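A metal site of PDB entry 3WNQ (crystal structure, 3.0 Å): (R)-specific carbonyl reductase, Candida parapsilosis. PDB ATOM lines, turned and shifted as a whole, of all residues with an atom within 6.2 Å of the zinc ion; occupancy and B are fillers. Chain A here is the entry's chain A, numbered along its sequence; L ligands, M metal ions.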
ATOM      1  N   GLY A  47     -31.244 -20.080   4.776  1.00  0.00           N
ATOM      2  CA  GLY A  47     -32.046 -20.650   3.725  1.00  0.00           C
ATOM      3  C   GLY A  47     -31.731 -22.054   3.338  1.00  0.00           C
ATOM      4  O   GLY A  47     -30.697 -22.645   3.696  1.00  0.00           O
ATOM      5  N   LEU A  48     -32.633 -22.580   2.543  1.00  0.00           N
ATOM      6  CA  LEU A  48     -32.540 -23.914   2.053  1.00  0.00           C
ATOM      7  C   LEU A  48     -32.847 -23.921   0.580  1.00  0.00           C
ATOM      8  O   LEU A  48     -33.892 -23.415   0.165  1.00  0.00           O
ATOM      9  CB  LEU A  48     -33.577 -24.759   2.774  1.00  0.00           C
ATOM     10  CG  LEU A  48     -33.820 -26.057   2.029  1.00  0.00           C
ATOM     11  CD1 LEU A  48     -32.450 -26.788   1.860  1.00  0.00           C
ATOM     12  CD2 LEU A  48     -34.866 -26.878   2.776  1.00  0.00           C
ATOM     13  N   CYS A  49     -31.957 -24.521  -0.206  1.00  0.00           N
ATOM     14  CA  CYS A  49     -32.189 -24.623  -1.637  1.00  0.00           C
ATOM     15  C   CYS A  49     -31.796 -25.997  -2.161  1.00  0.00           C
ATOM     16  O   CYS A  49     -31.221 -26.820  -1.428  1.00  0.00           O
ATOM     17  CB  CYS A  49     -31.418 -23.530  -2.386  1.00  0.00           C
ATOM     18  SG  CYS A  49     -29.724 -23.875  -2.676  1.00  0.00           S
ATOM     19  N   HIS A  50     -32.116 -26.258  -3.429  1.00  0.00           N
ATOM     20  CA  HIS A  50     -31.825 -27.552  -4.039  1.00  0.00           C
ATOM     21  C   HIS A  50     -30.397 -27.996  -3.796  1.00  0.00           C
ATOM     22  O   HIS A  50     -30.191 -29.170  -3.551  1.00  0.00           O
ATOM     23  CB  HIS A  50     -32.133 -27.557  -5.561  1.00  0.00           C
ATOM     24  CG  HIS A  50     -31.601 -28.757  -6.287  1.00  0.00           C
ATOM     25  ND1 HIS A  50     -30.292 -28.858  -6.702  1.00  0.00           N
ATOM     26  CD2 HIS A  50     -32.182 -29.931  -6.609  1.00  0.00           C
ATOM     27  CE1 HIS A  50     -30.082 -30.051  -7.248  1.00  0.00           C
ATOM     28  NE2 HIS A  50     -31.218 -30.711  -7.210  1.00  0.00           N
ATOM     29  N   SER A  51     -29.421 -27.091  -3.882  1.00  0.00           N
ATOM     30  CA  SER A  51     -28.008 -27.470  -3.664  1.00  0.00           C
ATOM     31  C   SER A  51     -27.904 -28.379  -2.445  1.00  0.00           C
ATOM     32  O   SER A  51     -27.368 -29.464  -2.528  1.00  0.00           O
ATOM     33  CB  SER A  51     -27.120 -26.261  -3.434  1.00  0.00           C
ATOM     34  OG  SER A  51     -26.658 -25.747  -4.655  1.00  0.00           O
ATOM     35  N   ASP A  52     -28.443 -27.914  -1.315  1.00  0.00           N
ATOM     36  CA  ASP A  52     -28.415 -28.662  -0.083  1.00  0.00           C
ATOM     37  C   ASP A  52     -28.845 -30.134  -0.293  1.00  0.00           C
ATOM     38  O   ASP A  52     -28.249 -31.053   0.267  1.00  0.00           O
ATOM     39  CB  ASP A  52     -29.279 -27.940   0.973  1.00  0.00           C
ATOM     40  CG  ASP A  52     -28.549 -26.734   1.614  1.00  0.00           C
ATOM     41  OD1 ASP A  52     -27.354 -26.878   2.048  1.00  0.00           O
ATOM     42  OD2 ASP A  52     -29.190 -25.652   1.705  1.00  0.00           O
ATOM     43  N   HIS A  70     -25.929 -22.822   3.451  1.00  0.00           N
ATOM     44  CA  HIS A  70     -24.997 -21.806   3.020  1.00  0.00           C
ATOM     45  C   HIS A  70     -25.626 -20.422   2.858  1.00  0.00           C
ATOM     46  O   HIS A  70     -24.925 -19.387   2.727  1.00  0.00           O
ATOM     47  CB  HIS A  70     -24.490 -22.250   1.708  1.00  0.00           C
ATOM     48  CG  HIS A  70     -25.560 -22.839   0.875  1.00  0.00           C
ATOM     49  ND1 HIS A  70     -26.151 -24.048   1.178  1.00  0.00           N
ATOM     50  CD2 HIS A  70     -26.212 -22.359  -0.214  1.00  0.00           C
ATOM     51  CE1 HIS A  70     -27.127 -24.279   0.318  1.00  0.00           C
ATOM     52  NE2 HIS A  70     -27.186 -23.276  -0.542  1.00  0.00           N
ATOM     53  N   GLU A  71     -26.945 -20.414   2.840  1.00  0.00           N
ATOM     54  CA  GLU A  71     -27.645 -19.164   2.666  1.00  0.00           C
ATOM     55  C   GLU A  71     -27.809 -18.659   4.062  1.00  0.00           C
ATOM     56  O   GLU A  71     -28.817 -18.840   4.661  1.00  0.00           O
ATOM     57  CB  GLU A  71     -28.967 -19.451   1.989  1.00  0.00           C
ATOM     58  CG  GLU A  71     -28.844 -20.589   0.983  1.00  0.00           C
ATOM     59  CD  GLU A  71     -29.742 -20.435  -0.198  1.00  0.00           C
ATOM     60  OE1 GLU A  71     -30.797 -19.751  -0.106  1.00  0.00           O
ATOM     61  OE2 GLU A  71     -29.392 -21.033  -1.241  1.00  0.00           O
ATOM     62  N   ASP A 159     -27.880 -16.785  -2.172  1.00  0.00           N
ATOM     63  CA  ASP A 159     -27.699 -17.697  -3.268  1.00  0.00           C
ATOM     64  C   ASP A 159     -28.743 -17.305  -4.310  1.00  0.00           C
ATOM     65  O   ASP A 159     -28.438 -16.910  -5.445  1.00  0.00           O
ATOM     66  CB  ASP A 159     -27.938 -19.148  -2.847  1.00  0.00           C
ATOM     67  CG  ASP A 159     -27.630 -20.146  -3.951  1.00  0.00           C
ATOM     68  OD1 ASP A 159     -27.971 -19.911  -5.142  1.00  0.00           O
ATOM     69  OD2 ASP A 159     -27.040 -21.204  -3.642  1.00  0.00           O
ATOM     70  N   ALA A 160     -30.009 -17.393  -3.901  1.00  0.00           N
ATOM     71  CA  ALA A 160     -31.086 -17.119  -4.828  1.00  0.00           C
ATOM     72  C   ALA A 160     -30.967 -15.871  -5.688  1.00  0.00           C
ATOM     73  O   ALA A 160     -31.381 -15.892  -6.879  1.00  0.00           O
ATOM     74  CB  ALA A 160     -32.409 -17.090  -4.081  1.00  0.00           C
ATOM     75  N   TRP A 291     -22.114 -18.963  -8.474  1.00  0.00           N
ATOM     76  CA  TRP A 291     -22.443 -18.238  -7.259  1.00  0.00           C
ATOM     77  C   TRP A 291     -22.052 -16.761  -7.374  1.00  0.00           C
ATOM     78  O   TRP A 291     -22.413 -16.133  -8.398  1.00  0.00           O
ATOM     79  CB  TRP A 291     -21.709 -18.858  -6.088  1.00  0.00           C
ATOM     80  CG  TRP A 291     -22.546 -18.937  -4.820  1.00  0.00           C
ATOM     81  CD1 TRP A 291     -23.569 -18.083  -4.439  1.00  0.00           C
ATOM     82  CD2 TRP A 291     -22.342 -19.838  -3.708  1.00  0.00           C
ATOM     83  NE1 TRP A 291     -23.998 -18.390  -3.161  1.00  0.00           N
ATOM     84  CE2 TRP A 291     -23.263 -19.462  -2.694  1.00  0.00           C
ATOM     85  CE3 TRP A 291     -21.474 -20.896  -3.471  1.00  0.00           C
ATOM     86  CZ2 TRP A 291     -23.328 -20.117  -1.466  1.00  0.00           C
ATOM     87  CZ3 TRP A 291     -21.539 -21.536  -2.251  1.00  0.00           C
ATOM     88  CH2 TRP A 291     -22.461 -21.144  -1.269  1.00  0.00           C
ATOM     89  N   ARG A 336     -38.570 -20.098  -1.846  1.00  0.00           N
ATOM     90  CA  ARG A 336     -37.505 -20.136  -0.866  1.00  0.00           C
ATOM     91  C   ARG A 336     -38.029 -20.210   0.594  1.00  0.00           C
ATOM     92  O   ARG A 336     -39.019 -19.569   0.932  1.00  0.00           O
ATOM     93  CB  ARG A 336     -36.600 -18.900  -1.090  1.00  0.00           C
ATOM     94  CG  ARG A 336     -35.684 -19.033  -2.252  1.00  0.00           C
ATOM     95  CD  ARG A 336     -34.836 -20.245  -2.001  1.00  0.00           C
ATOM     96  NE  ARG A 336     -34.098 -20.653  -3.173  1.00  0.00           N
ATOM     97  CZ  ARG A 336     -32.773 -20.694  -3.209  1.00  0.00           C
ATOM     98  NH1 ARG A 336     -32.089 -20.341  -2.115  1.00  0.00           N
ATOM     99  NH2 ARG A 336     -32.143 -21.063  -4.339  1.00  0.00           N
HETATM  100  C1  LIG L   1     -23.235 -25.206  -7.359  1.00  0.00           C
HETATM  101  C2  LIG L   1     -22.446 -26.142  -8.018  1.00  0.00           C
HETATM  102  C3  LIG L   1     -21.730 -27.071  -7.266  1.00  0.00           C
HETATM  103  C4  LIG L   1     -21.809 -27.050  -5.880  1.00  0.00           C
HETATM  104  C5  LIG L   1     -22.590 -26.103  -5.225  1.00  0.00           C
HETATM  105  C6  LIG L   1     -23.284 -25.150  -5.969  1.00  0.00           C
HETATM  106  C7  LIG L   1     -23.871 -24.066  -5.324  1.00  0.00           C
HETATM  107  O1  LIG L   1     -24.037 -24.068  -4.107  1.00  0.00           O
HETATM  108  C8  LIG L   1     -24.134 -22.809  -6.172  1.00  0.00           C
HETATM  109  O2  LIG L   1     -25.353 -22.169  -5.793  1.00  0.00           O
HETATM  110 ZN    ZN M   1     -28.528 -22.325  -2.058  1.00  0.00          ZN
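Within 4 Å of the zinc ion: Cys 49, His 70, Glu 71 and Asp 159.
The side-chain carboxylate (OE1) of Glu 71 is in salt-bridge range of the guanidinium group (NH1) of Arg 336. O of Glu 71 lies within hydrogen-bond range of N of Gly 47, at 2.7 Å. The backbone NH of Ser 51 lies close to the side-chain sulfur of Cys 49. A ring nitrogen (ND1) of His 70 lies close to the side-chain carboxylate (OD1) of Asp 52.
OD2 of Asp 159 lies close to O2 of the ligand. An oxygen (O1) of the ligand sits at hydrogen-bond distance from the side-chain hydroxyl (OG) of Ser 51, at 3.2 Å.
OE2 of Glu 71 is bound to the zinc ion, at 1.8 Å. The zinc ion is bound by the side-chain sulfur (SG) of Cys 49, at 2.1 Å. A ring nitrogen (NE2) of His 70 binds the zinc ion (2.2 Å). The zinc ion is bound by OD2 of Asp 159, at 2.4 Å.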
